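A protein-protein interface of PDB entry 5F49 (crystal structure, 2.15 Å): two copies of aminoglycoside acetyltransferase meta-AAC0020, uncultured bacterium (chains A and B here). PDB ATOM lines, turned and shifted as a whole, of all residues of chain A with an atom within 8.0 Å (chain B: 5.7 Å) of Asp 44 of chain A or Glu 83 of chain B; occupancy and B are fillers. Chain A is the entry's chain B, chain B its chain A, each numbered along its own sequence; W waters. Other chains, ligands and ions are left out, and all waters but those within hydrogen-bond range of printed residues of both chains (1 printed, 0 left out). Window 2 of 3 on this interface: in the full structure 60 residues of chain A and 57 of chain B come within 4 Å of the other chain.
The backbone carbonyl oxygen (O) of Gln 79 of chain B is in hydrogen-bond range of a ring nitrogen (NE2) of His 47 of chain A (2.7 Å).
The backbone carbonyl oxygen (O) of Ser 82 of chain B lies within hydrogen-bond range of a ring nitrogen (NE2) of His 47 of chain A.
The side-chain carboxylate (OD2) of Asp 44 of chain A sits close to the side-chain carboxylate (OE2) of Glu 83 of chain B, 2.8 Å away.
NE2 of Gln 79 of chain B is in hydrogen-bond range of O of Lys 84 of chain B (2.5 Å).
OG of Ser 82 of chain B is in hydrogen-bond range of N of Lys 84 of chain B, at 2.8 Å.
The side-chain carboxylate (OD1) of Asp 44 of chain A lies within hydrogen-bond range of the backbone NH (N) of His 47 of chain A (3.0 Å).
Among the printed residues, merely in contact across the chains: Pro 43 of chain A with Tyr 81 of chain B, Pro 43 of chain A with Ser 82 of chain B, His 47 of chain A with Glu 78 of chain B, His 47 of chain A with Glu 83 of chain B, Leu 51 of chain A with Glu 78 of chain B and Leu 51 of chain A with Gln 79 of chain B.
Of the printed residues of chain B, Asp 44 of chain A touches Glu 83 (2.8 Å).
Lys 50 of chain A touches none of the printed residues of chain B.
Printed residues of chain B within 4 Å of Leu 51 of chain A: Glu 78 (3.9 Å) and Gln 79 (3.6 Å).
Of the printed residues of chain A, Gln 79 of chain B touches His 47 (2.7 Å) and Leu 51 (3.6 Å).
Of the printed residues of chain A, Tyr 81 of chain B touches Pro 43 (3.7 Å).
Glu 83 of chain B touches two residues of chain A.
The nearest printed residue of chain B that does not touch Asp 44 of chain A is Ser 82 of chain B (7.3 Å).
The nearest residue of chain A that does not touch Glu 83 of chain B is Pro 43 of chain A (4.2 Å).
Printed residues of chain A that touch a printed residue of chain B: Pro 43, Asp 44, His 47 and Leu 51.
Hydrophobic or aromatic side chains of chain A within 4 Å of the printed part of chain B: Pro 43, His 47 and Leu 51.
Of the 7 printed residues of chain B, 5 touch a printed residue of chain A.
Printed residues of chain B that touch a printed residue of chain A: Glu 78, Gln 79, Tyr 81, Ser 82 and Glu 83.
Among the printed residues, 9 pairs touch across the chains.
Among the printed residues, no Asp or Glu carboxylate lies within 4 Å of a Lys or Arg side-chain nitrogen of the other chain.
No position is printed for both chains.
Of the 9 pairs that touch across the chains among the printed residues, none has its exchanged pair printed and touching as well.
Water W1 bridges the backbone carbonyl oxygen (O) of Tyr 81 of chain B (2.9 Å) and the backbone carbonyl oxygen (O) of Ser 41 of chain A (3.2 Å).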
ATOM      1  N   LEU A  21     -28.528 -25.518 -14.867  1.00  0.00           N
ATOM      2  CA  LEU A  21     -27.754 -25.624 -13.625  1.00  0.00           C
ATOM      3  C   LEU A  21     -26.824 -24.425 -13.366  1.00  0.00           C
ATOM      4  O   LEU A  21     -26.783 -23.930 -12.244  1.00  0.00           O
ATOM      5  CB  LEU A  21     -26.934 -26.916 -13.593  1.00  0.00           C
ATOM      6  CG  LEU A  21     -26.167 -27.130 -12.282  1.00  0.00           C
ATOM      7  CD1 LEU A  21     -27.140 -27.246 -11.110  1.00  0.00           C
ATOM      8  CD2 LEU A  21     -25.257 -28.348 -12.363  1.00  0.00           C
ATOM      9  N   ILE A  25     -26.803 -22.159  -9.904  1.00  0.00           N
ATOM     10  CA  ILE A  25     -25.634 -21.929  -9.068  1.00  0.00           C
ATOM     11  C   ILE A  25     -25.351 -20.429  -8.944  1.00  0.00           C
ATOM     12  O   ILE A  25     -24.996 -19.945  -7.863  1.00  0.00           O
ATOM     13  CB  ILE A  25     -24.406 -22.677  -9.626  1.00  0.00           C
ATOM     14  CG1 ILE A  25     -24.593 -24.190  -9.459  1.00  0.00           C
ATOM     15  CG2 ILE A  25     -23.119 -22.219  -8.951  1.00  0.00           C
ATOM     16  CD1 ILE A  25     -23.473 -25.035 -10.087  1.00  0.00           C
ATOM     17  N   ILE A  28     -27.760 -19.094  -6.382  1.00  0.00           N
ATOM     18  CA  ILE A  28     -27.310 -19.496  -5.053  1.00  0.00           C
ATOM     19  C   ILE A  28     -26.178 -18.581  -4.570  1.00  0.00           C
ATOM     20  O   ILE A  28     -26.141 -18.178  -3.401  1.00  0.00           O
ATOM     21  CB  ILE A  28     -26.843 -20.961  -5.046  1.00  0.00           C
ATOM     22  CG1 ILE A  28     -28.022 -21.889  -5.349  1.00  0.00           C
ATOM     23  CG2 ILE A  28     -26.214 -21.318  -3.713  1.00  0.00           C
ATOM     24  CD1 ILE A  28     -27.636 -23.344  -5.549  1.00  0.00           C
ATOM     25  N   SER A  41     -20.413 -23.502   2.160  1.00  0.00           N
ATOM     26  CA  SER A  41     -19.926 -24.535   1.249  1.00  0.00           C
ATOM     27  C   SER A  41     -21.073 -25.027   0.374  1.00  0.00           C
ATOM     28  O   SER A  41     -21.979 -25.707   0.855  1.00  0.00           O
ATOM     29  CB  SER A  41     -19.314 -25.704   2.018  1.00  0.00           C
ATOM     30  OG  SER A  41     -18.174 -25.294   2.752  1.00  0.00           O
ATOM     31  N   ILE A  42     -21.042 -24.675  -0.906  1.00  0.00           N
ATOM     32  CA  ILE A  42     -22.112 -25.066  -1.817  1.00  0.00           C
ATOM     33  C   ILE A  42     -22.135 -26.593  -1.973  1.00  0.00           C
ATOM     34  O   ILE A  42     -21.093 -27.227  -2.080  1.00  0.00           O
ATOM     35  CB  ILE A  42     -21.960 -24.362  -3.198  1.00  0.00           C
ATOM     36  CG1 ILE A  42     -23.219 -24.545  -4.051  1.00  0.00           C
ATOM     37  CG2 ILE A  42     -20.706 -24.837  -3.935  1.00  0.00           C
ATOM     38  CD1 ILE A  42     -23.305 -23.596  -5.220  1.00  0.00           C
ATOM     39  N   PRO A  43     -23.334 -27.193  -1.938  1.00  0.00           N
ATOM     40  CA  PRO A  43     -23.483 -28.632  -2.203  1.00  0.00           C
ATOM     41  C   PRO A  43     -22.975 -28.997  -3.594  1.00  0.00           C
ATOM     42  O   PRO A  43     -22.880 -28.107  -4.439  1.00  0.00           O
ATOM     43  CB  PRO A  43     -24.993 -28.852  -2.098  1.00  0.00           C
ATOM     44  CG  PRO A  43     -25.469 -27.739  -1.199  1.00  0.00           C
ATOM     45  CD  PRO A  43     -24.604 -26.564  -1.533  1.00  0.00           C
ATOM     46  N   ASP A  44     -22.663 -30.267  -3.839  1.00  0.00           N
ATOM     47  CA  ASP A  44     -22.124 -30.647  -5.142  1.00  0.00           C
ATOM     48  C   ASP A  44     -23.176 -30.517  -6.242  1.00  0.00           C
ATOM     49  O   ASP A  44     -24.381 -30.492  -5.977  1.00  0.00           O
ATOM     50  CB  ASP A  44     -21.537 -32.066  -5.112  1.00  0.00           C
ATOM     51  CG  ASP A  44     -22.451 -33.081  -4.452  1.00  0.00           C
ATOM     52  OD1 ASP A  44     -23.652 -33.118  -4.779  1.00  0.00           O
ATOM     53  OD2 ASP A  44     -21.952 -33.858  -3.611  1.00  0.00           O
ATOM     54  N   SER A  45     -22.702 -30.405  -7.479  1.00  0.00           N
ATOM     55  CA  SER A  45     -23.578 -30.212  -8.635  1.00  0.00           C
ATOM     56  C   SER A  45     -24.517 -31.389  -8.842  1.00  0.00           C
ATOM     57  O   SER A  45     -25.615 -31.219  -9.360  1.00  0.00           O
ATOM     58  CB  SER A  45     -22.751 -29.985  -9.901  1.00  0.00           C
ATOM     59  OG  SER A  45     -22.053 -28.755  -9.836  1.00  0.00           O
ATOM     60  N   GLU A  46     -24.082 -32.582  -8.449  1.00  0.00           N
ATOM     61  CA  GLU A  46     -24.941 -33.755  -8.534  1.00  0.00           C
ATOM     62  C   GLU A  46     -26.223 -33.523  -7.739  1.00  0.00           C
ATOM     63  O   GLU A  46     -27.328 -33.771  -8.229  1.00  0.00           O
ATOM     64  CB  GLU A  46     -24.225 -35.001  -8.019  1.00  0.00           C
ATOM     65  CG  GLU A  46     -25.118 -36.230  -7.975  1.00  0.00           C
ATOM     66  CD  GLU A  46     -24.433 -37.442  -7.370  1.00  0.00           C
ATOM     67  OE1 GLU A  46     -23.414 -37.268  -6.669  1.00  0.00           O
ATOM     68  OE2 GLU A  46     -24.914 -38.572  -7.599  1.00  0.00           O
ATOM     69  N   HIS A  47     -26.064 -33.022  -6.519  1.00  0.00           N
ATOM     70  CA  HIS A  47     -27.202 -32.772  -5.648  1.00  0.00           C
ATOM     71  C   HIS A  47     -28.060 -31.612  -6.146  1.00  0.00           C
ATOM     72  O   HIS A  47     -29.286 -31.682  -6.104  1.00  0.00           O
ATOM     73  CB  HIS A  47     -26.733 -32.493  -4.220  1.00  0.00           C
ATOM     74  CG  HIS A  47     -27.823 -31.999  -3.323  1.00  0.00           C
ATOM     75  ND1 HIS A  47     -28.720 -32.844  -2.703  1.00  0.00           N
ATOM     76  CD2 HIS A  47     -28.180 -30.744  -2.960  1.00  0.00           C
ATOM     77  CE1 HIS A  47     -29.573 -32.132  -1.991  1.00  0.00           C
ATOM     78  NE2 HIS A  47     -29.268 -30.853  -2.131  1.00  0.00           N
ATOM     79  N   LEU A  48     -27.420 -30.544  -6.613  1.00  0.00           N
ATOM     80  CA  LEU A  48     -28.155 -29.381  -7.109  1.00  0.00           C
ATOM     81  C   LEU A  48     -28.931 -29.710  -8.390  1.00  0.00           C
ATOM     82  O   LEU A  48     -30.041 -29.224  -8.596  1.00  0.00           O
ATOM     83  CB  LEU A  48     -27.201 -28.210  -7.353  1.00  0.00           C
ATOM     84  CG  LEU A  48     -26.562 -27.588  -6.103  1.00  0.00           C
ATOM     85  CD1 LEU A  48     -25.708 -26.388  -6.476  1.00  0.00           C
ATOM     86  CD2 LEU A  48     -27.631 -27.203  -5.086  1.00  0.00           C
ATOM     87  N   GLN A  49     -28.342 -30.538  -9.247  1.00  0.00           N
ATOM     88  CA  GLN A  49     -29.005 -30.936 -10.483  1.00  0.00           C
ATOM     89  C   GLN A  49     -30.258 -31.765 -10.191  1.00  0.00           C
ATOM     90  O   GLN A  49     -31.303 -31.569 -10.812  1.00  0.00           O
ATOM     91  CB  GLN A  49     -28.052 -31.727 -11.384  1.00  0.00           C
ATOM     92  CG  GLN A  49     -28.677 -32.136 -12.712  1.00  0.00           C
ATOM     93  CD  GLN A  49     -29.014 -30.939 -13.597  1.00  0.00           C
ATOM     94  OE1 GLN A  49     -28.120 -30.270 -14.123  1.00  0.00           O
ATOM     95  NE2 GLN A  49     -30.308 -30.668 -13.765  1.00  0.00           N
ATOM     96  N   LYS A  50     -30.156 -32.681  -9.235  1.00  0.00           N
ATOM     97  CA  LYS A  50     -31.297 -33.516  -8.874  1.00  0.00           C
ATOM     98  C   LYS A  50     -32.425 -32.690  -8.271  1.00  0.00           C
ATOM     99  O   LYS A  50     -33.602 -32.984  -8.501  1.00  0.00           O
ATOM    100  CB  LYS A  50     -30.874 -34.626  -7.908  1.00  0.00           C
ATOM    101  CG  LYS A  50     -30.004 -35.690  -8.566  1.00  0.00           C
ATOM    102  CD  LYS A  50     -29.793 -36.903  -7.671  1.00  0.00           C
ATOM    103  CE  LYS A  50     -28.948 -36.560  -6.455  1.00  0.00           C
ATOM    104  NZ  LYS A  50     -28.624 -37.776  -5.653  1.00  0.00           N
ATOM    105  N   LEU A  51     -32.066 -31.657  -7.511  1.00  0.00           N
ATOM    106  CA  LEU A  51     -33.061 -30.737  -6.964  1.00  0.00           C
ATOM    107  C   LEU A  51     -33.755 -29.976  -8.089  1.00  0.00           C
ATOM    108  O   LEU A  51     -34.982 -29.901  -8.136  1.00  0.00           O
ATOM    109  CB  LEU A  51     -32.409 -29.758  -5.980  1.00  0.00           C
ATOM    110  CG  LEU A  51     -33.223 -28.541  -5.534  1.00  0.00           C
ATOM    111  CD1 LEU A  51     -34.564 -28.953  -4.948  1.00  0.00           C
ATOM    112  CD2 LEU A  51     -32.418 -27.730  -4.520  1.00  0.00           C
ATOM    113  N   GLU B  78     -36.224 -30.314  -0.060  1.00  0.00           N
ATOM    114  CA  GLU B  78     -34.825 -30.489  -0.421  1.00  0.00           C
ATOM    115  C   GLU B  78     -34.154 -29.123  -0.550  1.00  0.00           C
ATOM    116  O   GLU B  78     -34.740 -28.191  -1.099  1.00  0.00           O
ATOM    117  CB  GLU B  78     -34.708 -31.273  -1.726  1.00  0.00           C
ATOM    118  CG  GLU B  78     -33.329 -31.848  -1.989  1.00  0.00           C
ATOM    119  CD  GLU B  78     -33.060 -33.103  -1.175  1.00  0.00           C
ATOM    120  OE1 GLU B  78     -31.996 -33.173  -0.523  1.00  0.00           O
ATOM    121  OE2 GLU B  78     -33.914 -34.016  -1.195  1.00  0.00           O
ATOM    122  N   GLN B  79     -32.930 -29.006  -0.045  1.00  0.00           N
ATOM    123  CA  GLN B  79     -32.247 -27.715   0.000  1.00  0.00           C
ATOM    124  C   GLN B  79     -31.153 -27.557  -1.050  1.00  0.00           C
ATOM    125  O   GLN B  79     -30.590 -28.539  -1.548  1.00  0.00           O
ATOM    126  CB  GLN B  79     -31.622 -27.485   1.375  1.00  0.00           C
ATOM    127  CG  GLN B  79     -32.574 -27.537   2.546  1.00  0.00           C
ATOM    128  CD  GLN B  79     -31.893 -27.095   3.833  1.00  0.00           C
ATOM    129  OE1 GLN B  79     -31.801 -25.901   4.120  1.00  0.00           O
ATOM    130  NE2 GLN B  79     -31.396 -28.059   4.603  1.00  0.00           N
ATOM    131  N   TYR B  81     -28.898 -25.183  -0.042  1.00  0.00           N
ATOM    132  CA  TYR B  81     -27.904 -24.718   0.925  1.00  0.00           C
ATOM    133  C   TYR B  81     -27.156 -25.894   1.550  1.00  0.00           C
ATOM    134  O   TYR B  81     -26.071 -25.731   2.097  1.00  0.00           O
ATOM    135  CB  TYR B  81     -28.566 -23.883   2.027  1.00  0.00           C
ATOM    136  CG  TYR B  81     -29.067 -22.527   1.580  1.00  0.00           C
ATOM    137  CD1 TYR B  81     -28.335 -21.753   0.690  1.00  0.00           C
ATOM    138  CD2 TYR B  81     -30.277 -22.021   2.050  1.00  0.00           C
ATOM    139  CE1 TYR B  81     -28.789 -20.514   0.282  1.00  0.00           C
ATOM    140  CE2 TYR B  81     -30.742 -20.776   1.645  1.00  0.00           C
ATOM    141  CZ  TYR B  81     -29.994 -20.031   0.757  1.00  0.00           C
ATOM    142  OH  TYR B  81     -30.452 -18.798   0.349  1.00  0.00           O
ATOM    143  N   SER B  82     -27.746 -27.080   1.464  1.00  0.00           N
ATOM    144  CA  SER B  82     -27.184 -28.275   2.083  1.00  0.00           C
ATOM    145  C   SER B  82     -27.702 -29.531   1.398  1.00  0.00           C
ATOM    146  O   SER B  82     -28.716 -29.487   0.703  1.00  0.00           O
ATOM    147  CB  SER B  82     -27.532 -28.316   3.577  1.00  0.00           C
ATOM    148  OG  SER B  82     -27.441 -29.634   4.096  1.00  0.00           O
ATOM    149  N   GLU B  83     -27.013 -30.648   1.602  1.00  0.00           N
ATOM    150  CA  GLU B  83     -27.494 -31.928   1.091  1.00  0.00           C
ATOM    151  C   GLU B  83     -28.555 -32.521   2.012  1.00  0.00           C
ATOM    152  O   GLU B  83     -29.303 -33.413   1.621  1.00  0.00           O
ATOM    153  CB  GLU B  83     -26.339 -32.919   0.924  1.00  0.00           C
ATOM    154  CG  GLU B  83     -25.385 -32.586  -0.201  1.00  0.00           C
ATOM    155  CD  GLU B  83     -24.855 -33.827  -0.893  1.00  0.00           C
ATOM    156  OE1 GLU B  83     -25.441 -34.914  -0.699  1.00  0.00           O
ATOM    157  OE2 GLU B  83     -23.857 -33.717  -1.632  1.00  0.00           O
ATOM    158  N   LYS B  84     -28.617 -32.024   3.240  1.00  0.00           N
ATOM    159  CA  LYS B  84     -29.580 -32.527   4.207  1.00  0.00           C
ATOM    160  C   LYS B  84     -30.893 -31.746   4.114  1.00  0.00           C
ATOM    161  O   LYS B  84     -30.907 -30.523   4.227  1.00  0.00           O
ATOM    162  CB  LYS B  84     -28.984 -32.454   5.611  1.00  0.00           C
ATOM    163  CG  LYS B  84     -27.710 -33.286   5.738  1.00  0.00           C
ATOM    164  CD  LYS B  84     -26.799 -32.797   6.848  1.00  0.00           C
ATOM    165  CE  LYS B  84     -27.335 -33.144   8.219  1.00  0.00           C
ATOM    166  NZ  LYS B  84     -26.348 -32.755   9.270  1.00  0.00           N
ATOM    167  N   PRO B  85     -32.002 -32.459   3.880  1.00  0.00           N
ATOM    168  CA  PRO B  85     -33.290 -31.809   3.628  1.00  0.00           C
ATOM    169  C   PRO B  85     -33.897 -31.167   4.873  1.00  0.00           C
ATOM    170  O   PRO B  85     -33.463 -31.439   5.995  1.00  0.00           O
ATOM    171  CB  PRO B  85     -34.176 -32.961   3.133  1.00  0.00           C
ATOM    172  CG  PRO B  85     -33.227 -34.075   2.775  1.00  0.00           C
ATOM    173  CD  PRO B  85     -32.079 -33.918   3.706  1.00  0.00           C
HETATM  174  O   HOH W   1     -23.701 -26.887   3.293  1.00  0.00           O
